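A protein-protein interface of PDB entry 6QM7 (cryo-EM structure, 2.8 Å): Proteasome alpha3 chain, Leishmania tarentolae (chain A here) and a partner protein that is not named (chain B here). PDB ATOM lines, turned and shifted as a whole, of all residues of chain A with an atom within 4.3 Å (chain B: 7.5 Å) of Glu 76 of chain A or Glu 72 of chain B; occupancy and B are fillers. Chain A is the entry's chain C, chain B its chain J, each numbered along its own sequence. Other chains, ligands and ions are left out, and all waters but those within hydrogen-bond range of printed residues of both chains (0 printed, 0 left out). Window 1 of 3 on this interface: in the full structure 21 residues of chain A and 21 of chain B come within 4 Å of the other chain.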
ATOM      1  N   LYS A  73      -0.679   2.300 -12.110  1.00  0.00           N
ATOM      2  CA  LYS A  73      -1.958   1.795 -11.563  1.00  0.00           C
ATOM      3  C   LYS A  73      -3.035   2.077 -12.601  1.00  0.00           C
ATOM      4  O   LYS A  73      -3.094   3.210 -13.048  1.00  0.00           O
ATOM      5  CB  LYS A  73      -2.281   2.468 -10.230  1.00  0.00           C
ATOM      6  CG  LYS A  73      -3.696   2.245  -9.732  1.00  0.00           C
ATOM      7  CD  LYS A  73      -3.823   2.067  -8.243  1.00  0.00           C
ATOM      8  CE  LYS A  73      -3.961   3.362  -7.480  1.00  0.00           C
ATOM      9  NZ  LYS A  73      -3.144   3.328  -6.241  1.00  0.00           N
ATOM     10  N   ALA A  75      -6.338   0.657 -11.952  1.00  0.00           N
ATOM     11  CA  ALA A  75      -7.405   0.794 -10.944  1.00  0.00           C
ATOM     12  C   ALA A  75      -6.902   0.156  -9.655  1.00  0.00           C
ATOM     13  O   ALA A  75      -5.844  -0.455  -9.709  1.00  0.00           O
ATOM     14  CB  ALA A  75      -8.661   0.140 -11.445  1.00  0.00           C
ATOM     15  N   GLU A  76      -7.638   0.287  -8.551  1.00  0.00           N
ATOM     16  CA  GLU A  76      -7.183  -0.156  -7.203  1.00  0.00           C
ATOM     17  C   GLU A  76      -6.599  -1.568  -7.303  1.00  0.00           C
ATOM     18  O   GLU A  76      -5.501  -1.779  -6.756  1.00  0.00           O
ATOM     19  CB  GLU A  76      -8.325  -0.072  -6.186  1.00  0.00           C
ATOM     20  CG  GLU A  76      -8.510   1.334  -5.612  1.00  0.00           C
ATOM     21  CD  GLU A  76      -9.898   1.667  -5.063  1.00  0.00           C
ATOM     22  OE1 GLU A  76     -10.301   2.853  -5.155  1.00  0.00           O
ATOM     23  OE2 GLU A  76     -10.576   0.749  -4.535  1.00  0.00           O
ATOM     24  N   HIS A  77      -7.273  -2.444  -8.050  1.00  0.00           N
ATOM     25  CA  HIS A  77      -6.975  -3.894  -8.188  1.00  0.00           C
ATOM     26  C   HIS A  77      -6.237  -4.246  -9.485  1.00  0.00           C
ATOM     27  O   HIS A  77      -6.120  -5.445  -9.745  1.00  0.00           O
ATOM     28  CB  HIS A  77      -8.279  -4.678  -8.137  1.00  0.00           C
ATOM     29  CG  HIS A  77      -9.133  -4.486  -9.336  1.00  0.00           C
ATOM     30  ND1 HIS A  77      -9.769  -3.281  -9.601  1.00  0.00           N
ATOM     31  CD2 HIS A  77      -9.478  -5.330 -10.330  1.00  0.00           C
ATOM     32  CE1 HIS A  77     -10.446  -3.386 -10.729  1.00  0.00           C
ATOM     33  NE2 HIS A  77     -10.284  -4.636 -11.197  1.00  0.00           N
ATOM     34  N   ILE A  78      -5.793  -3.277 -10.289  1.00  0.00           N
ATOM     35  CA  ILE A  78      -5.071  -3.549 -11.570  1.00  0.00           C
ATOM     36  C   ILE A  78      -3.903  -2.580 -11.697  1.00  0.00           C
ATOM     37  O   ILE A  78      -4.125  -1.373 -11.655  1.00  0.00           O
ATOM     38  CB  ILE A  78      -5.964  -3.436 -12.825  1.00  0.00           C
ATOM     39  CG1 ILE A  78      -7.391  -3.931 -12.596  1.00  0.00           C
ATOM     40  CG2 ILE A  78      -5.308  -4.137 -14.007  1.00  0.00           C
ATOM     41  CD1 ILE A  78      -8.220  -3.988 -13.851  1.00  0.00           C
ATOM     42  N   LEU A 101     -12.986   1.883 -15.039  1.00  0.00           N
ATOM     43  CA  LEU A 101     -13.946   2.732 -14.296  1.00  0.00           C
ATOM     44  C   LEU A 101     -15.315   2.689 -14.962  1.00  0.00           C
ATOM     45  O   LEU A 101     -16.300   2.813 -14.212  1.00  0.00           O
ATOM     46  CB  LEU A 101     -13.425   4.166 -14.207  1.00  0.00           C
ATOM     47  CG  LEU A 101     -12.183   4.368 -13.337  1.00  0.00           C
ATOM     48  CD1 LEU A 101     -12.011   5.840 -13.004  1.00  0.00           C
ATOM     49  CD2 LEU A 101     -12.217   3.536 -12.053  1.00  0.00           C
ATOM     50  N   MET A 221       1.371  -5.936  -6.755  1.00  0.00           N
ATOM     51  CA  MET A 221      -0.072  -6.190  -6.578  1.00  0.00           C
ATOM     52  C   MET A 221      -0.210  -7.232  -5.477  1.00  0.00           C
ATOM     53  O   MET A 221       0.318  -8.339  -5.668  1.00  0.00           O
ATOM     54  CB  MET A 221      -0.689  -6.739  -7.861  1.00  0.00           C
ATOM     55  CG  MET A 221      -2.187  -6.736  -7.839  1.00  0.00           C
ATOM     56  SD  MET A 221      -2.825  -5.052  -8.047  1.00  0.00           S
ATOM     57  CE  MET A 221      -3.826  -5.022  -6.566  1.00  0.00           C
ATOM     58  N   PRO A 244      -7.371  -5.635  -2.611  1.00  0.00           N
ATOM     59  CA  PRO A 244      -6.120  -5.522  -3.359  1.00  0.00           C
ATOM     60  C   PRO A 244      -5.571  -4.091  -3.320  1.00  0.00           C
ATOM     61  O   PRO A 244      -6.352  -3.173  -3.349  1.00  0.00           O
ATOM     62  CB  PRO A 244      -6.513  -5.918  -4.784  1.00  0.00           C
ATOM     63  CG  PRO A 244      -7.986  -5.654  -4.860  1.00  0.00           C
ATOM     64  CD  PRO A 244      -8.513  -5.953  -3.480  1.00  0.00           C
ATOM     65  N   ARG A 245      -4.250  -3.956  -3.225  1.00  0.00           N
ATOM     66  CA  ARG A 245      -3.539  -2.655  -3.244  1.00  0.00           C
ATOM     67  C   ARG A 245      -2.283  -2.798  -4.101  1.00  0.00           C
ATOM     68  O   ARG A 245      -1.395  -3.583  -3.740  1.00  0.00           O
ATOM     69  CB  ARG A 245      -3.191  -2.195  -1.827  1.00  0.00           C
ATOM     70  CG  ARG A 245      -2.935  -0.698  -1.688  1.00  0.00           C
ATOM     71  CD  ARG A 245      -2.539  -0.312  -0.265  1.00  0.00           C
ATOM     72  NE  ARG A 245      -1.358  -1.076   0.144  1.00  0.00           N
ATOM     73  CZ  ARG A 245      -0.079  -0.713  -0.013  1.00  0.00           C
ATOM     74  NH1 ARG A 245       0.249   0.458  -0.540  1.00  0.00           N
ATOM     75  NH2 ARG A 245       0.881  -1.537   0.380  1.00  0.00           N
ATOM     76  N   PHE A 246      -2.251  -2.071  -5.214  1.00  0.00           N
ATOM     77  CA  PHE A 246      -1.047  -1.842  -6.042  1.00  0.00           C
ATOM     78  C   PHE A 246      -0.108  -0.914  -5.276  1.00  0.00           C
ATOM     79  O   PHE A 246      -0.574   0.148  -4.816  1.00  0.00           O
ATOM     80  CB  PHE A 246      -1.438  -1.223  -7.382  1.00  0.00           C
ATOM     81  CG  PHE A 246      -0.335  -1.227  -8.407  1.00  0.00           C
ATOM     82  CD1 PHE A 246       0.158  -2.424  -8.903  1.00  0.00           C
ATOM     83  CD2 PHE A 246       0.189  -0.040  -8.891  1.00  0.00           C
ATOM     84  CE1 PHE A 246       1.156  -2.437  -9.866  1.00  0.00           C
ATOM     85  CE2 PHE A 246       1.190  -0.051  -9.848  1.00  0.00           C
ATOM     86  CZ  PHE A 246       1.667  -1.250 -10.338  1.00  0.00           C
ATOM     87  N   VAL B  44     -18.541   9.153   0.775  1.00  0.00           N
ATOM     88  CA  VAL B  44     -17.183   9.589   1.196  1.00  0.00           C
ATOM     89  C   VAL B  44     -16.274   9.580  -0.030  1.00  0.00           C
ATOM     90  O   VAL B  44     -15.931   8.487  -0.514  1.00  0.00           O
ATOM     91  CB  VAL B  44     -16.643   8.706   2.324  1.00  0.00           C
ATOM     92  CG1 VAL B  44     -15.194   9.030   2.643  1.00  0.00           C
ATOM     93  CG2 VAL B  44     -17.515   8.851   3.554  1.00  0.00           C
ATOM     94  N   VAL B  45     -15.907  10.770  -0.491  1.00  0.00           N
ATOM     95  CA  VAL B  45     -15.000  10.942  -1.650  1.00  0.00           C
ATOM     96  C   VAL B  45     -13.599  10.565  -1.178  1.00  0.00           C
ATOM     97  O   VAL B  45     -12.948   9.733  -1.832  1.00  0.00           O
ATOM     98  CB  VAL B  45     -15.047  12.374  -2.199  1.00  0.00           C
ATOM     99  CG1 VAL B  45     -14.148  12.514  -3.416  1.00  0.00           C
ATOM    100  CG2 VAL B  45     -16.463  12.829  -2.520  1.00  0.00           C
ATOM    101  N   LYS B  66     -21.655   8.669 -11.203  1.00  0.00           N
ATOM    102  CA  LYS B  66     -20.963   9.574 -12.148  1.00  0.00           C
ATOM    103  C   LYS B  66     -19.856  10.296 -11.404  1.00  0.00           C
ATOM    104  O   LYS B  66     -18.800  10.444 -11.977  1.00  0.00           O
ATOM    105  CB  LYS B  66     -21.886  10.651 -12.706  1.00  0.00           C
ATOM    106  CG  LYS B  66     -22.797  10.223 -13.841  1.00  0.00           C
ATOM    107  CD  LYS B  66     -23.376  11.422 -14.582  1.00  0.00           C
ATOM    108  CE  LYS B  66     -23.299  11.269 -16.084  1.00  0.00           C
ATOM    109  NZ  LYS B  66     -23.864   9.965 -16.530  1.00  0.00           N
ATOM    110  N   VAL B  67     -20.126  10.731 -10.180  1.00  0.00           N
ATOM    111  CA  VAL B  67     -19.142  11.452  -9.330  1.00  0.00           C
ATOM    112  C   VAL B  67     -18.041  10.476  -8.933  1.00  0.00           C
ATOM    113  O   VAL B  67     -16.886  10.891  -8.952  1.00  0.00           O
ATOM    114  CB  VAL B  67     -19.811  12.078  -8.093  1.00  0.00           C
ATOM    115  CG1 VAL B  67     -18.801  12.471  -7.024  1.00  0.00           C
ATOM    116  CG2 VAL B  67     -20.668  13.270  -8.489  1.00  0.00           C
ATOM    117  N   GLN B  68     -18.402   9.258  -8.541  1.00  0.00           N
ATOM    118  CA  GLN B  68     -17.431   8.230  -8.099  1.00  0.00           C
ATOM    119  C   GLN B  68     -16.494   7.897  -9.261  1.00  0.00           C
ATOM    120  O   GLN B  68     -15.318   7.631  -9.003  1.00  0.00           O
ATOM    121  CB  GLN B  68     -18.158   6.984  -7.601  1.00  0.00           C
ATOM    122  CG  GLN B  68     -17.269   5.968  -6.891  1.00  0.00           C
ATOM    123  CD  GLN B  68     -17.860   4.585  -7.013  1.00  0.00           C
ATOM    124  OE1 GLN B  68     -18.937   4.304  -6.484  1.00  0.00           O
ATOM    125  NE2 GLN B  68     -17.178   3.716  -7.745  1.00  0.00           N
ATOM    126  N   PHE B  69     -16.993   7.923 -10.491  1.00  0.00           N
ATOM    127  CA  PHE B  69     -16.193   7.756 -11.730  1.00  0.00           C
ATOM    128  C   PHE B  69     -15.201   8.919 -11.828  1.00  0.00           C
ATOM    129  O   PHE B  69     -13.995   8.695 -11.976  1.00  0.00           O
ATOM    130  CB  PHE B  69     -17.133   7.663 -12.933  1.00  0.00           C
ATOM    131  CG  PHE B  69     -16.453   7.612 -14.274  1.00  0.00           C
ATOM    132  CD1 PHE B  69     -16.244   6.410 -14.912  1.00  0.00           C
ATOM    133  CD2 PHE B  69     -16.056   8.780 -14.908  1.00  0.00           C
ATOM    134  CE1 PHE B  69     -15.616   6.370 -16.144  1.00  0.00           C
ATOM    135  CE2 PHE B  69     -15.427   8.740 -16.138  1.00  0.00           C
ATOM    136  CZ  PHE B  69     -15.201   7.534 -16.747  1.00  0.00           C
ATOM    137  N   ARG B  70     -15.710  10.139 -11.723  1.00  0.00           N
ATOM    138  CA  ARG B  70     -14.925  11.375 -11.933  1.00  0.00           C
ATOM    139  C   ARG B  70     -13.854  11.507 -10.846  1.00  0.00           C
ATOM    140  O   ARG B  70     -12.724  11.864 -11.202  1.00  0.00           O
ATOM    141  CB  ARG B  70     -15.857  12.583 -11.966  1.00  0.00           C
ATOM    142  CG  ARG B  70     -16.786  12.623 -13.173  1.00  0.00           C
ATOM    143  CD  ARG B  70     -16.052  12.927 -14.448  1.00  0.00           C
ATOM    144  NE  ARG B  70     -15.359  14.191 -14.275  1.00  0.00           N
ATOM    145  CZ  ARG B  70     -15.915  15.394 -14.407  1.00  0.00           C
ATOM    146  NH1 ARG B  70     -17.192  15.520 -14.749  1.00  0.00           N
ATOM    147  NH2 ARG B  70     -15.174  16.472 -14.205  1.00  0.00           N
ATOM    148  N   THR B  71     -14.183  11.219  -9.585  1.00  0.00           N
ATOM    149  CA  THR B  71     -13.252  11.355  -8.439  1.00  0.00           C
ATOM    150  C   THR B  71     -12.204  10.253  -8.455  1.00  0.00           C
ATOM    151  O   THR B  71     -11.100  10.534  -7.961  1.00  0.00           O
ATOM    152  CB  THR B  71     -13.925  11.271  -7.072  1.00  0.00           C
ATOM    153  OG1 THR B  71     -14.534   9.986  -6.967  1.00  0.00           O
ATOM    154  CG2 THR B  71     -14.928  12.377  -6.844  1.00  0.00           C
ATOM    155  N   GLU B  72     -12.527   9.053  -8.943  1.00  0.00           N
ATOM    156  CA  GLU B  72     -11.530   7.955  -9.070  1.00  0.00           C
ATOM    157  C   GLU B  72     -10.608   8.214 -10.264  1.00  0.00           C
ATOM    158  O   GLU B  72      -9.424   7.880 -10.143  1.00  0.00           O
ATOM    159  CB  GLU B  72     -12.195   6.583  -9.195  1.00  0.00           C
ATOM    160  CG  GLU B  72     -12.726   6.031  -7.878  1.00  0.00           C
ATOM    161  CD  GLU B  72     -11.709   5.840  -6.752  1.00  0.00           C
ATOM    162  OE1 GLU B  72     -12.147   5.761  -5.573  1.00  0.00           O
ATOM    163  OE2 GLU B  72     -10.482   5.768  -7.044  1.00  0.00           O
ATOM    164  N   MET B  73     -11.131   8.741 -11.375  1.00  0.00           N
ATOM    165  CA  MET B  73     -10.326   9.097 -12.576  1.00  0.00           C
ATOM    166  C   MET B  73      -9.331  10.179 -12.180  1.00  0.00           C
ATOM    167  O   MET B  73      -8.180  10.107 -12.607  1.00  0.00           O
ATOM    168  CB  MET B  73     -11.164   9.645 -13.740  1.00  0.00           C
ATOM    169  CG  MET B  73     -11.189   8.782 -15.004  1.00  0.00           C
ATOM    170  SD  MET B  73      -9.756   7.697 -15.257  1.00  0.00           S
ATOM    171  CE  MET B  73      -8.899   8.529 -16.595  1.00  0.00           C
ATOM    172  N   TYR B  74      -9.808  11.179 -11.445  1.00  0.00           N
ATOM    173  CA  TYR B  74      -9.011  12.316 -10.932  1.00  0.00           C
ATOM    174  C   TYR B  74      -7.830  11.750 -10.156  1.00  0.00           C
ATOM    175  O   TYR B  74      -6.703  12.103 -10.439  1.00  0.00           O
ATOM    176  CB  TYR B  74      -9.879  13.186 -10.028  1.00  0.00           C
ATOM    177  CG  TYR B  74      -9.256  14.478  -9.585  1.00  0.00           C
ATOM    178  CD1 TYR B  74      -9.576  15.666 -10.218  1.00  0.00           C
ATOM    179  CD2 TYR B  74      -8.383  14.529  -8.514  1.00  0.00           C
ATOM    180  CE1 TYR B  74      -9.034  16.873  -9.807  1.00  0.00           C
ATOM    181  CE2 TYR B  74      -7.825  15.725  -8.094  1.00  0.00           C
ATOM    182  CZ  TYR B  74      -8.151  16.908  -8.743  1.00  0.00           C
ATOM    183  OH  TYR B  74      -7.627  18.112  -8.346  1.00  0.00           O
ATOM    184  N   LYS B  75      -8.129  10.855  -9.225  1.00  0.00           N
ATOM    185  CA  LYS B  75      -7.172  10.248  -8.272  1.00  0.00           C
ATOM    186  C   LYS B  75      -6.067   9.528  -9.057  1.00  0.00           C
ATOM    187  O   LYS B  75      -4.916   9.493  -8.561  1.00  0.00           O
ATOM    188  CB  LYS B  75      -7.939   9.303  -7.338  1.00  0.00           C
ATOM    189  CG  LYS B  75      -7.597   9.379  -5.857  1.00  0.00           C
ATOM    190  CD  LYS B  75      -6.526   8.391  -5.414  1.00  0.00           C
ATOM    191  CE  LYS B  75      -6.433   8.244  -3.907  1.00  0.00           C
ATOM    192  NZ  LYS B  75      -5.769   9.413  -3.273  1.00  0.00           N
ATOM    193  N   LEU B  76      -6.398   8.944 -10.207  1.00  0.00           N
ATOM    194  CA  LEU B  76      -5.427   8.206 -11.051  1.00  0.00           C
ATOM    195  C   LEU B  76      -4.597   9.201 -11.852  1.00  0.00           C
ATOM    196  O   LEU B  76      -3.358   9.145 -11.759  1.00  0.00           O
ATOM    197  CB  LEU B  76      -6.160   7.264 -12.001  1.00  0.00           C
ATOM    198  CG  LEU B  76      -6.783   6.040 -11.346  1.00  0.00           C
ATOM    199  CD1 LEU B  76      -7.813   5.398 -12.265  1.00  0.00           C
ATOM    200  CD2 LEU B  76      -5.711   5.035 -10.962  1.00  0.00           C
ATOM    201  N   ARG B  77      -5.265  10.042 -12.638  1.00  0.00           N
ATOM    202  CA  ARG B  77      -4.620  11.072 -13.483  1.00  0.00           C
ATOM    203  C   ARG B  77      -3.773  11.979 -12.584  1.00  0.00           C
ATOM    204  O   ARG B  77      -2.544  11.979 -12.737  1.00  0.00           O
ATOM    205  CB  ARG B  77      -5.672  11.850 -14.275  1.00  0.00           C
ATOM    206  CG  ARG B  77      -6.169  11.156 -15.538  1.00  0.00           C
ATOM    207  CD  ARG B  77      -6.761  12.147 -16.535  1.00  0.00           C
ATOM    208  NE  ARG B  77      -7.742  12.964 -15.824  1.00  0.00           N
ATOM    209  CZ  ARG B  77      -9.069  12.768 -15.783  1.00  0.00           C
ATOM    210  NH1 ARG B  77      -9.819  13.579 -15.045  1.00  0.00           N
ATOM    211  NH2 ARG B  77      -9.648  11.792 -16.473  1.00  0.00           N
ATOM    212  N   GLU B  78      -4.406  12.668 -11.641  1.00  0.00           N
ATOM    213  CA  GLU B  78      -3.799  13.756 -10.827  1.00  0.00           C
ATOM    214  C   GLU B  78      -2.831  13.213  -9.784  1.00  0.00           C
ATOM    215  O   GLU B  78      -2.006  14.015  -9.310  1.00  0.00           O
ATOM    216  CB  GLU B  78      -4.862  14.547 -10.071  1.00  0.00           C
ATOM    217  CG  GLU B  78      -5.932  15.110 -10.988  1.00  0.00           C
ATOM    218  CD  GLU B  78      -5.908  16.603 -11.246  1.00  0.00           C
ATOM    219  OE1 GLU B  78      -6.515  17.004 -12.255  1.00  0.00           O
ATOM    220  OE2 GLU B  78      -5.317  17.350 -10.432  1.00  0.00           O
ATOM    221  N   ARG B  80      -3.415  12.443  -6.726  1.00  0.00           N
ATOM    222  CA  ARG B  80      -3.729  13.081  -5.422  1.00  0.00           C
ATOM    223  C   ARG B  80      -5.231  13.019  -5.185  1.00  0.00           C
ATOM    224  O   ARG B  80      -5.969  12.795  -6.144  1.00  0.00           O
ATOM    225  CB  ARG B  80      -3.284  14.546  -5.351  1.00  0.00           C
ATOM    226  CG  ARG B  80      -3.796  15.411  -6.491  1.00  0.00           C
ATOM    227  CD  ARG B  80      -3.674  16.893  -6.209  1.00  0.00           C
ATOM    228  NE  ARG B  80      -4.268  17.688  -7.278  1.00  0.00           N
ATOM    229  CZ  ARG B  80      -4.421  19.010  -7.253  1.00  0.00           C
ATOM    230  NH1 ARG B  80      -4.017  19.713  -6.206  1.00  0.00           N
ATOM    231  NH2 ARG B  80      -4.974  19.633  -8.281  1.00  0.00           N
ATOM    232  N   ILE B  82      -8.736  14.644  -4.632  1.00  0.00           N
ATOM    233  CA  ILE B  82      -9.432  15.912  -4.980  1.00  0.00           C
ATOM    234  C   ILE B  82      -9.727  16.661  -3.670  1.00  0.00           C
ATOM    235  O   ILE B  82      -9.927  15.998  -2.630  1.00  0.00           O
ATOM    236  CB  ILE B  82     -10.663  15.627  -5.865  1.00  0.00           C
ATOM    237  CG1 ILE B  82     -11.172  16.889  -6.563  1.00  0.00           C
ATOM    238  CG2 ILE B  82     -11.771  14.932  -5.097  1.00  0.00           C
ATOM    239  CD1 ILE B  82     -12.133  16.611  -7.700  1.00  0.00           C
ATOM    240  N   MET B  90     -16.234  20.822  -9.592  1.00  0.00           N
ATOM    241  CA  MET B  90     -16.448  19.664 -10.496  1.00  0.00           C
ATOM    242  C   MET B  90     -17.928  19.311 -10.521  1.00  0.00           C
ATOM    243  O   MET B  90     -18.457  19.072 -11.605  1.00  0.00           O
ATOM    244  CB  MET B  90     -15.676  18.429 -10.037  1.00  0.00           C
ATOM    245  CG  MET B  90     -15.825  17.256 -10.983  1.00  0.00           C
ATOM    246  SD  MET B  90     -15.109  15.763 -10.298  1.00  0.00           S
ATOM    247  CE  MET B  90     -16.450  15.313  -9.200  1.00  0.00           C
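The side-chain carboxylate (OE1) of Glu 76 of chain A sits close to the side-chain carboxylate (OE1) of Glu 72 of chain B, at 3.5 Å.
Leu 76 of chain B touches Lys 73 of chain A. Leu 101 of chain A touches Phe 69 of chain B (CD1 to O, 3.6 Å). Leu 101 of chain A touches Glu 72 of chain B. CD1 of Leu 101 of chain A touches N of Met 73 of chain B (3.4 Å).
Of the printed residues of chain B, Lys 73 of chain A touches Leu 76. Glu 76 of chain A touches one residue of chain B. Of the printed residues of chain B, Leu 101 of chain A touches Phe 69, Glu 72 and Met 73. Of the printed residues of chain A, Phe 69 of chain B touches Leu 101. Glu 72 of chain B touches two residues of chain A. Of the printed residues of chain A, Met 73 of chain B touches Leu 101. Of the printed residues of chain A, Leu 76 of chain B touches Lys 73. The nearest printed residue of chain A that does not touch Glu 72 of chain B is Lys 73 of chain A (7.0 Å). The nearest printed residue of chain A that does not touch Met 73 of chain B is Lys 73 of chain A (8.3 Å).
Of the 18 printed residues of chain B, 4 touch a printed residue of chain A. Of the 10 printed residues of chain A, 3 touch a printed residue of chain B. Printed residues of chain A that touch a printed residue of chain B: Lys 73, Glu 76 and Leu 101. Among the printed residues, no Asp or Glu carboxylate lies within 4 Å of a Lys or Arg side-chain nitrogen of the other chain.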
